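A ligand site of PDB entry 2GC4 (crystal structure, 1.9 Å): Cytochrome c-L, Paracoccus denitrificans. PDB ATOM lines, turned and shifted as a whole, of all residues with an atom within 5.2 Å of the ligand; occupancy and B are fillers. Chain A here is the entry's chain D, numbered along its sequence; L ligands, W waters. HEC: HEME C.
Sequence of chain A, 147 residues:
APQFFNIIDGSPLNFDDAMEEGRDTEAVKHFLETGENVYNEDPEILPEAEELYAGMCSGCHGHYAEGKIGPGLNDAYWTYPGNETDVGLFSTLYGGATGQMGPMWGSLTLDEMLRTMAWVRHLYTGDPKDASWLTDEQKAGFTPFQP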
ATOM      1  N   TYR A  53     -30.235   3.274   1.671  1.00  0.00           N
ATOM      2  CA  TYR A  53     -28.969   2.744   2.149  1.00  0.00           C
ATOM      3  C   TYR A  53     -27.903   3.830   2.201  1.00  0.00           C
ATOM      4  O   TYR A  53     -27.166   3.949   3.181  1.00  0.00           O
ATOM      5  CB  TYR A  53     -28.492   1.626   1.216  1.00  0.00           C
ATOM      6  CG  TYR A  53     -27.130   1.088   1.587  1.00  0.00           C
ATOM      7  CD1 TYR A  53     -26.993   0.092   2.561  1.00  0.00           C
ATOM      8  CD2 TYR A  53     -25.979   1.619   1.025  1.00  0.00           C
ATOM      9  CE1 TYR A  53     -25.725  -0.364   2.950  1.00  0.00           C
ATOM     10  CE2 TYR A  53     -24.718   1.169   1.409  1.00  0.00           C
ATOM     11  CZ  TYR A  53     -24.601   0.189   2.368  1.00  0.00           C
ATOM     12  OH  TYR A  53     -23.340  -0.203   2.756  1.00  0.00           O
ATOM     13  N   MET A  56     -28.645   6.234   5.230  1.00  0.00           N
ATOM     14  CA  MET A  56     -28.666   5.608   6.552  1.00  0.00           C
ATOM     15  C   MET A  56     -27.555   4.616   6.902  1.00  0.00           C
ATOM     16  O   MET A  56     -27.290   4.390   8.071  1.00  0.00           O
ATOM     17  CB  MET A  56     -29.999   4.884   6.746  1.00  0.00           C
ATOM     18  CG  MET A  56     -31.206   5.792   6.855  1.00  0.00           C
ATOM     19  SD  MET A  56     -31.604   6.130   8.565  1.00  0.00           S
ATOM     20  CE  MET A  56     -30.348   7.259   8.995  1.00  0.00           C
ATOM     21  N   CYS A  57     -26.908   4.036   5.890  1.00  0.00           N
ATOM     22  CA  CYS A  57     -25.907   3.007   6.148  1.00  0.00           C
ATOM     23  C   CYS A  57     -24.511   3.177   5.560  1.00  0.00           C
ATOM     24  O   CYS A  57     -23.560   2.624   6.108  1.00  0.00           O
ATOM     25  CB  CYS A  57     -26.430   1.655   5.665  1.00  0.00           C
ATOM     26  SG  CYS A  57     -28.241   1.442   5.681  1.00  0.00           S
ATOM     27  N   CYS A  60     -21.109   4.068   7.557  1.00  0.00           N
ATOM     28  CA  CYS A  60     -20.406   3.058   8.347  1.00  0.00           C
ATOM     29  C   CYS A  60     -20.027   1.782   7.607  1.00  0.00           C
ATOM     30  O   CYS A  60     -18.971   1.214   7.845  1.00  0.00           O
ATOM     31  CB  CYS A  60     -21.238   2.676   9.570  1.00  0.00           C
ATOM     32  SG  CYS A  60     -21.523   4.010  10.776  1.00  0.00           S
ATOM     33  N   HIS A  61     -20.900   1.322   6.711  1.00  0.00           N
ATOM     34  CA  HIS A  61     -20.650   0.087   5.996  1.00  0.00           C
ATOM     35  C   HIS A  61     -20.042   0.228   4.599  1.00  0.00           C
ATOM     36  O   HIS A  61     -19.789  -0.771   3.934  1.00  0.00           O
ATOM     37  CB  HIS A  61     -21.945  -0.733   5.945  1.00  0.00           C
ATOM     38  CG  HIS A  61     -22.349  -1.284   7.278  1.00  0.00           C
ATOM     39  ND1 HIS A  61     -21.630  -2.287   7.866  1.00  0.00           N
ATOM     40  CD2 HIS A  61     -23.418  -0.772   7.909  1.00  0.00           C
ATOM     41  CE1 HIS A  61     -22.314  -2.440   9.048  1.00  0.00           C
ATOM     42  NE2 HIS A  61     -23.412  -1.525   9.091  1.00  0.00           N
ATOM     43  N   ILE A  69     -15.750   1.751   8.590  1.00  0.00           N
ATOM     44  CA  ILE A  69     -15.461   1.732  10.018  1.00  0.00           C
ATOM     45  C   ILE A  69     -16.356   0.668  10.635  1.00  0.00           C
ATOM     46  O   ILE A  69     -16.188   0.290  11.797  1.00  0.00           O
ATOM     47  CB  ILE A  69     -15.711   3.116  10.713  1.00  0.00           C
ATOM     48  CG1 ILE A  69     -17.197   3.420  10.819  1.00  0.00           C
ATOM     49  CG2 ILE A  69     -14.986   4.206   9.934  1.00  0.00           C
ATOM     50  CD1 ILE A  69     -17.794   3.969   9.572  1.00  0.00           C
ATOM     51  N   GLY A  70     -17.304   0.181   9.837  1.00  0.00           N
ATOM     52  CA  GLY A  70     -18.206  -0.876  10.264  1.00  0.00           C
ATOM     53  C   GLY A  70     -17.891  -2.057   9.350  1.00  0.00           C
ATOM     54  O   GLY A  70     -17.242  -1.862   8.328  1.00  0.00           O
ATOM     55  N   PRO A  71     -18.349  -3.283   9.679  1.00  0.00           N
ATOM     56  CA  PRO A  71     -18.081  -4.463   8.853  1.00  0.00           C
ATOM     57  C   PRO A  71     -18.782  -4.538   7.498  1.00  0.00           C
ATOM     58  O   PRO A  71     -19.876  -3.989   7.313  1.00  0.00           O
ATOM     59  CB  PRO A  71     -18.506  -5.605   9.767  1.00  0.00           C
ATOM     60  CG  PRO A  71     -19.672  -5.016  10.498  1.00  0.00           C
ATOM     61  CD  PRO A  71     -19.145  -3.634  10.864  1.00  0.00           C
ATOM     62  N   GLY A  72     -18.138  -5.211   6.552  1.00  0.00           N
ATOM     63  CA  GLY A  72     -18.727  -5.369   5.232  1.00  0.00           C
ATOM     64  C   GLY A  72     -19.984  -6.207   5.316  1.00  0.00           C
ATOM     65  O   GLY A  72     -20.137  -6.992   6.256  1.00  0.00           O
ATOM     66  N   LEU A  73     -20.880  -6.046   4.355  1.00  0.00           N
ATOM     67  CA  LEU A  73     -22.134  -6.806   4.334  1.00  0.00           C
ATOM     68  C   LEU A  73     -22.357  -7.402   2.955  1.00  0.00           C
ATOM     69  O   LEU A  73     -23.466  -7.832   2.638  1.00  0.00           O
ATOM     70  CB  LEU A  73     -23.321  -5.881   4.639  1.00  0.00           C
ATOM     71  CG  LEU A  73     -23.220  -4.907   5.825  1.00  0.00           C
ATOM     72  CD1 LEU A  73     -24.384  -3.927   5.745  1.00  0.00           C
ATOM     73  CD2 LEU A  73     -23.218  -5.668   7.130  1.00  0.00           C
ATOM     74  N   TYR A  77     -19.974 -14.158   4.520  1.00  0.00           N
ATOM     75  CA  TYR A  77     -19.706 -14.241   5.949  1.00  0.00           C
ATOM     76  C   TYR A  77     -20.588 -13.290   6.756  1.00  0.00           C
ATOM     77  O   TYR A  77     -20.751 -12.123   6.382  1.00  0.00           O
ATOM     78  CB  TYR A  77     -18.235 -13.925   6.262  1.00  0.00           C
ATOM     79  CG  TYR A  77     -17.985 -13.910   7.763  1.00  0.00           C
ATOM     80  CD1 TYR A  77     -17.949 -15.095   8.486  1.00  0.00           C
ATOM     81  CD2 TYR A  77     -17.894 -12.705   8.454  1.00  0.00           C
ATOM     82  CE1 TYR A  77     -17.836 -15.095   9.877  1.00  0.00           C
ATOM     83  CE2 TYR A  77     -17.781 -12.688   9.843  1.00  0.00           C
ATOM     84  CZ  TYR A  77     -17.758 -13.886  10.550  1.00  0.00           C
ATOM     85  OH  TYR A  77     -17.672 -13.888  11.915  1.00  0.00           O
ATOM     86  N   TRP A  78     -21.131 -13.786   7.853  1.00  0.00           N
ATOM     87  CA  TRP A  78     -21.965 -12.975   8.727  1.00  0.00           C
ATOM     88  C   TRP A  78     -21.584 -13.200  10.188  1.00  0.00           C
ATOM     89  O   TRP A  78     -21.517 -14.344  10.643  1.00  0.00           O
ATOM     90  CB  TRP A  78     -23.449 -13.320   8.543  1.00  0.00           C
ATOM     91  CG  TRP A  78     -23.967 -13.072   7.160  1.00  0.00           C
ATOM     92  CD1 TRP A  78     -24.147 -14.006   6.173  1.00  0.00           C
ATOM     93  CD2 TRP A  78     -24.407 -11.821   6.612  1.00  0.00           C
ATOM     94  NE1 TRP A  78     -24.665 -13.412   5.048  1.00  0.00           N
ATOM     95  CE2 TRP A  78     -24.832 -12.072   5.287  1.00  0.00           C
ATOM     96  CE3 TRP A  78     -24.472 -10.523   7.112  1.00  0.00           C
ATOM     97  CZ2 TRP A  78     -25.322 -11.065   4.457  1.00  0.00           C
ATOM     98  CZ3 TRP A  78     -24.954  -9.510   6.279  1.00  0.00           C
ATOM     99  CH2 TRP A  78     -25.374  -9.788   4.977  1.00  0.00           C
ATOM    100  N   THR A  79     -21.331 -12.124  10.917  1.00  0.00           N
ATOM    101  CA  THR A  79     -20.985 -12.232  12.330  1.00  0.00           C
ATOM    102  C   THR A  79     -22.154 -12.938  13.013  1.00  0.00           C
ATOM    103  O   THR A  79     -21.958 -13.754  13.917  1.00  0.00           O
ATOM    104  CB  THR A  79     -20.779 -10.847  12.954  1.00  0.00           C
ATOM    105  OG1 THR A  79     -19.621 -10.235  12.389  1.00  0.00           O
ATOM    106  CG2 THR A  79     -20.620 -10.958  14.466  1.00  0.00           C
ATOM    107  N   TYR A  80     -23.356 -12.602  12.583  1.00  0.00           N
ATOM    108  CA  TYR A  80     -24.577 -13.204  13.124  1.00  0.00           C
ATOM    109  C   TYR A  80     -25.084 -14.076  11.990  1.00  0.00           C
ATOM    110  O   TYR A  80     -25.663 -13.591  11.020  1.00  0.00           O
ATOM    111  CB  TYR A  80     -25.576 -12.100  13.483  1.00  0.00           C
ATOM    112  CG  TYR A  80     -25.031 -11.181  14.553  1.00  0.00           C
ATOM    113  CD1 TYR A  80     -24.919 -11.604  15.867  1.00  0.00           C
ATOM    114  CD2 TYR A  80     -24.567  -9.909  14.224  1.00  0.00           C
ATOM    115  CE1 TYR A  80     -24.342 -10.796  16.849  1.00  0.00           C
ATOM    116  CE2 TYR A  80     -23.982  -9.085  15.193  1.00  0.00           C
ATOM    117  CZ  TYR A  80     -23.877  -9.537  16.506  1.00  0.00           C
ATOM    118  OH  TYR A  80     -23.291  -8.754  17.469  1.00  0.00           O
ATOM    119  N   ASN A  83     -28.202 -13.828   9.611  1.00  0.00           N
ATOM    120  CA  ASN A  83     -28.345 -12.783   8.596  1.00  0.00           C
ATOM    121  C   ASN A  83     -28.290 -13.268   7.150  1.00  0.00           C
ATOM    122  O   ASN A  83     -28.456 -12.471   6.224  1.00  0.00           O
ATOM    123  CB  ASN A  83     -27.336 -11.659   8.835  1.00  0.00           C
ATOM    124  CG  ASN A  83     -27.702 -10.802  10.020  1.00  0.00           C
ATOM    125  OD1 ASN A  83     -28.884 -10.697  10.360  1.00  0.00           O
ATOM    126  ND2 ASN A  83     -26.719 -10.168  10.643  1.00  0.00           N
ATOM    127  N   LEU A  89     -31.903 -10.948   8.940  1.00  0.00           N
ATOM    128  CA  LEU A  89     -31.451  -9.604   8.565  1.00  0.00           C
ATOM    129  C   LEU A  89     -32.437  -8.582   9.124  1.00  0.00           C
ATOM    130  O   LEU A  89     -32.035  -7.566   9.700  1.00  0.00           O
ATOM    131  CB  LEU A  89     -31.355  -9.493   7.038  1.00  0.00           C
ATOM    132  CG  LEU A  89     -30.966  -8.132   6.462  1.00  0.00           C
ATOM    133  CD1 LEU A  89     -29.679  -7.656   7.115  1.00  0.00           C
ATOM    134  CD2 LEU A  89     -30.776  -8.239   4.953  1.00  0.00           C
ATOM    135  N   THR A  92     -32.031  -8.088  12.818  1.00  0.00           N
ATOM    136  CA  THR A  92     -30.854  -7.298  13.150  1.00  0.00           C
ATOM    137  C   THR A  92     -31.172  -5.811  13.063  1.00  0.00           C
ATOM    138  O   THR A  92     -30.811  -5.040  13.961  1.00  0.00           O
ATOM    139  CB  THR A  92     -29.681  -7.621  12.208  1.00  0.00           C
ATOM    140  OG1 THR A  92     -29.310  -8.997  12.362  1.00  0.00           O
ATOM    141  CG2 THR A  92     -28.482  -6.734  12.512  1.00  0.00           C
ATOM    142  N   LEU A  93     -31.839  -5.405  11.985  1.00  0.00           N
ATOM    143  CA  LEU A  93     -32.182  -3.990  11.812  1.00  0.00           C
ATOM    144  C   LEU A  93     -33.223  -3.488  12.806  1.00  0.00           C
ATOM    145  O   LEU A  93     -33.097  -2.383  13.334  1.00  0.00           O
ATOM    146  CB  LEU A  93     -32.713  -3.733  10.395  1.00  0.00           C
ATOM    147  CG  LEU A  93     -31.765  -3.891   9.213  1.00  0.00           C
ATOM    148  CD1 LEU A  93     -32.480  -3.502   7.938  1.00  0.00           C
ATOM    149  CD2 LEU A  93     -30.555  -3.024   9.417  1.00  0.00           C
ATOM    150  N   ALA A  97     -28.029  -4.586  17.002  1.00  0.00           N
ATOM    151  CA  ALA A  97     -26.946  -5.516  17.337  1.00  0.00           C
ATOM    152  C   ALA A  97     -26.257  -4.898  18.548  1.00  0.00           C
ATOM    153  O   ALA A  97     -26.915  -4.609  19.542  1.00  0.00           O
ATOM    154  CB  ALA A  97     -25.970  -5.651  16.162  1.00  0.00           C
ATOM    155  N   THR A  98     -24.945  -4.686  18.458  1.00  0.00           N
ATOM    156  CA  THR A  98     -24.223  -4.064  19.563  1.00  0.00           C
ATOM    157  C   THR A  98     -23.576  -2.768  19.105  1.00  0.00           C
ATOM    158  O   THR A  98     -23.544  -2.461  17.908  1.00  0.00           O
ATOM    159  CB  THR A  98     -23.136  -4.974  20.143  1.00  0.00           C
ATOM    160  OG1 THR A  98     -22.057  -5.094  19.209  1.00  0.00           O
ATOM    161  CG2 THR A  98     -23.691  -6.347  20.447  1.00  0.00           C
ATOM    162  N   GLN A 100     -22.757   0.858  18.006  1.00  0.00           N
ATOM    163  CA  GLN A 100     -23.507   1.873  17.288  1.00  0.00           C
ATOM    164  C   GLN A 100     -24.531   1.324  16.303  1.00  0.00           C
ATOM    165  O   GLN A 100     -25.202   2.075  15.615  1.00  0.00           O
ATOM    166  CB  GLN A 100     -22.536   2.820  16.577  1.00  0.00           C
ATOM    167  CG  GLN A 100     -21.725   3.667  17.536  1.00  0.00           C
ATOM    168  CD  GLN A 100     -20.754   4.586  16.836  1.00  0.00           C
ATOM    169  OE1 GLN A 100     -19.811   4.129  16.179  1.00  0.00           O
ATOM    170  NE2 GLN A 100     -20.967   5.882  16.966  1.00  0.00           N
ATOM    171  N   MET A 101     -24.633  -0.003  16.237  1.00  0.00           N
ATOM    172  CA  MET A 101     -25.612  -0.635  15.363  1.00  0.00           C
ATOM    173  C   MET A 101     -26.848  -0.910  16.229  1.00  0.00           C
ATOM    174  O   MET A 101     -27.064  -2.032  16.678  1.00  0.00           O
ATOM    175  CB  MET A 101     -25.056  -1.948  14.806  1.00  0.00           C
ATOM    176  CG  MET A 101     -25.973  -2.627  13.792  1.00  0.00           C
ATOM    177  SD  MET A 101     -26.318  -1.595  12.347  1.00  0.00           S
ATOM    178  CE  MET A 101     -27.930  -2.223  11.910  1.00  0.00           C
ATOM    179  N   MET A 104     -33.544   0.185  14.489  1.00  0.00           N
ATOM    180  CA  MET A 104     -33.905   1.141  13.460  1.00  0.00           C
ATOM    181  C   MET A 104     -35.400   1.476  13.448  1.00  0.00           C
ATOM    182  O   MET A 104     -35.852   2.256  12.602  1.00  0.00           O
ATOM    183  CB  MET A 104     -33.527   0.593  12.082  1.00  0.00           C
ATOM    184  CG  MET A 104     -32.058   0.251  11.875  1.00  0.00           C
ATOM    185  SD  MET A 104     -31.022   1.701  11.568  1.00  0.00           S
ATOM    186  CE  MET A 104     -29.485   1.172  12.319  1.00  0.00           C
ATOM    187  N   LEU A 108     -36.945   4.046  10.629  1.00  0.00           N
ATOM    188  CA  LEU A 108     -37.444   3.428   9.414  1.00  0.00           C
ATOM    189  C   LEU A 108     -38.785   2.739   9.616  1.00  0.00           C
ATOM    190  O   LEU A 108     -39.021   2.123  10.658  1.00  0.00           O
ATOM    191  CB  LEU A 108     -36.439   2.392   8.893  1.00  0.00           C
ATOM    192  CG  LEU A 108     -35.058   2.881   8.454  1.00  0.00           C
ATOM    193  CD1 LEU A 108     -34.149   1.684   8.222  1.00  0.00           C
ATOM    194  CD2 LEU A 108     -35.189   3.714   7.187  1.00  0.00           C
ATOM    195  N   THR A 116     -34.628  -1.374   2.261  1.00  0.00           N
ATOM    196  CA  THR A 116     -33.204  -1.207   2.540  1.00  0.00           C
ATOM    197  C   THR A 116     -32.519  -2.572   2.464  1.00  0.00           C
ATOM    198  O   THR A 116     -31.427  -2.696   1.900  1.00  0.00           O
ATOM    199  CB  THR A 116     -32.983  -0.602   3.950  1.00  0.00           C
ATOM    200  OG1 THR A 116     -33.609   0.686   4.002  1.00  0.00           O
ATOM    201  CG2 THR A 116     -31.488  -0.435   4.231  1.00  0.00           C
ATOM    202  N   VAL A 120     -29.175  -4.253   0.216  1.00  0.00           N
ATOM    203  CA  VAL A 120     -28.040  -4.965   0.801  1.00  0.00           C
ATOM    204  C   VAL A 120     -27.873  -6.295   0.057  1.00  0.00           C
ATOM    205  O   VAL A 120     -26.754  -6.700  -0.256  1.00  0.00           O
ATOM    206  CB  VAL A 120     -28.255  -5.223   2.314  1.00  0.00           C
ATOM    207  CG1 VAL A 120     -27.173  -6.172   2.835  1.00  0.00           C
ATOM    208  CG2 VAL A 120     -28.197  -3.902   3.076  1.00  0.00           C
HETATM  209 FE   HEC L   1     -24.720  -1.661  10.647  1.00  0.00          FE
HETATM  210  CHA HEC L   1     -23.483  -4.526  11.883  1.00  0.00           C
HETATM  211  CHB HEC L   1     -26.768  -3.461   8.601  1.00  0.00           C
HETATM  212  CHC HEC L   1     -26.202   1.242   9.538  1.00  0.00           C
HETATM  213  CHD HEC L   1     -22.497   0.168  12.416  1.00  0.00           C
HETATM  214  NA  HEC L   1     -25.075  -3.642  10.321  1.00  0.00           N
HETATM  215  C1A HEC L   1     -24.477  -4.677  10.944  1.00  0.00           C
HETATM  216  C2A HEC L   1     -25.036  -5.924  10.463  1.00  0.00           C
HETATM  217  C3A HEC L   1     -25.934  -5.618   9.523  1.00  0.00           C
HETATM  218  C4A HEC L   1     -25.983  -4.183   9.427  1.00  0.00           C
HETATM  219  CMA HEC L   1     -26.821  -6.600   8.687  1.00  0.00           C
HETATM  220  CAA HEC L   1     -24.601  -7.340  10.980  1.00  0.00           C
HETATM  221  CBA HEC L   1     -23.514  -7.931  10.090  1.00  0.00           C
HETATM  222  CGA HEC L   1     -23.091  -9.349  10.372  1.00  0.00           C
HETATM  223  O1A HEC L   1     -23.963 -10.159  10.908  1.00  0.00           O
HETATM  224  O2A HEC L   1     -21.957  -9.632  10.049  1.00  0.00           O
HETATM  225  NB  HEC L   1     -26.169  -1.203   9.320  1.00  0.00           N
HETATM  226  C1B HEC L   1     -26.895  -2.100   8.536  1.00  0.00           C
HETATM  227  C2B HEC L   1     -27.812  -1.401   7.645  1.00  0.00           C
HETATM  228  C3B HEC L   1     -27.700  -0.076   7.962  1.00  0.00           C
HETATM  229  C4B HEC L   1     -26.673   0.052   8.973  1.00  0.00           C
HETATM  230  CMB HEC L   1     -28.769  -2.079   6.563  1.00  0.00           C
HETATM  231  CAB HEC L   1     -28.471   1.132   7.407  1.00  0.00           C
HETATM  232  CBB HEC L   1     -29.970   1.133   7.899  1.00  0.00           C
HETATM  233  NC  HEC L   1     -24.420   0.306  10.956  1.00  0.00           N
HETATM  234  C1C HEC L   1     -25.135   1.360  10.416  1.00  0.00           C
HETATM  235  C2C HEC L   1     -24.567   2.649  10.849  1.00  0.00           C
HETATM  236  C3C HEC L   1     -23.498   2.339  11.604  1.00  0.00           C
HETATM  237  C4C HEC L   1     -23.407   0.892  11.687  1.00  0.00           C
HETATM  238  CMC HEC L   1     -25.133   4.061  10.434  1.00  0.00           C
HETATM  239  CAC HEC L   1     -22.462   3.287  12.228  1.00  0.00           C
HETATM  240  CBC HEC L   1     -22.902   4.280  13.321  1.00  0.00           C
HETATM  241  ND  HEC L   1     -23.274  -2.096  11.903  1.00  0.00           N
HETATM  242  C1D HEC L   1     -22.409  -1.204  12.566  1.00  0.00           C
HETATM  243  C2D HEC L   1     -21.454  -1.918  13.407  1.00  0.00           C
HETATM  244  C3D HEC L   1     -21.773  -3.256  13.287  1.00  0.00           C
HETATM  245  C4D HEC L   1     -22.873  -3.351  12.336  1.00  0.00           C
HETATM  246  CMD HEC L   1     -20.313  -1.239  14.287  1.00  0.00           C
HETATM  247  CAD HEC L   1     -21.121  -4.475  14.002  1.00  0.00           C
HETATM  248  CBD HEC L   1     -22.124  -4.811  15.230  1.00  0.00           C
HETATM  249  CGD HEC L   1     -21.839  -6.019  16.089  1.00  0.00           C
HETATM  250  O1D HEC L   1     -22.618  -6.280  17.017  1.00  0.00           O
HETATM  251  O2D HEC L   1     -20.902  -6.724  15.784  1.00  0.00           O
HETATM  252  O   HOH W   1     -19.858  -0.094  17.515  1.00  0.00           O
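CAB of the ligand is bonded to SG of Cys 57.
SG of Cys 60 is covalently linked to CAC of the ligand (1.9 Å).
A ring nitrogen (NE2) of His 61 is bound to an iron atom (FE) of the ligand (2.0 Å).
FE of the ligand is bound by SD of Met 101 (2.3 Å).
An oxygen (O1D) of the ligand sits at hydrogen-bond distance from the backbone NH of Thr 98, at 3.2 Å.
The side-chain hydroxyl (OG1) of Thr 98 sits at hydrogen-bond distance from an oxygen (O1D) of the ligand, at 2.6 Å.
The backbone NH (N) of Tyr 80 is in hydrogen-bond range of an oxygen (O1A) of the ligand, 3.0 Å away.
OH of Tyr 80 is in hydrogen-bond range of O1D of the ligand (2.6 Å).
The backbone NH (N) of Thr 79 lies within hydrogen-bond range of an oxygen (O2A) of the ligand, 2.7 Å away.
An oxygen (O2A) of the ligand is in hydrogen-bond range of the side-chain hydroxyl of Thr 79, 3.4 Å away.
The side-chain amide nitrogen (ND2) of Asn 83 is in hydrogen-bond range of an oxygen (O1A) of the ligand, at 2.8 Å.
The backbone carbonyl oxygen (O) of Cys 60 lies within hydrogen-bond range of the backbone NH (N) of Gly 70 (2.8 Å).
O of Cys 60 lies within hydrogen-bond range of N of Ile 69 (3.3 Å).
ND1 of His 61 is in hydrogen-bond range of O of Pro 71, 2.5 Å away.
OD1 of Asn 83 sits close to N of Leu 89, 3.3 Å away.
OD1 of Asn 83 lies within hydrogen-bond range of OG1 of Thr 92 (2.7 Å).
N of Met 104 is in hydrogen-bond range of O of Leu 93 (2.9 Å).
Merely in contact with the ligand: Met 56 (3.2 Å), Pro 71 (3.6 Å), Leu 73 (3.6 Å), Trp 78 (3.6 Å), Leu 89 (3.4 Å), Leu 93 (3.5 Å), Ala 97 (3.5 Å), Gln 100 (3.6 Å), Met 104 (3.9 Å), Thr 116 (3.9 Å) and Val 120 (3.98 Å).
Within 4 Å of the ligand: Met 56, Cys 57, Cys 60, His 61, Pro 71, Leu 73, Trp 78, Thr 79, Tyr 80, Asn 83, Leu 89, Leu 93, Ala 97, Thr 98, Gln 100, Met 101, Met 104, Thr 116 and Val 120.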
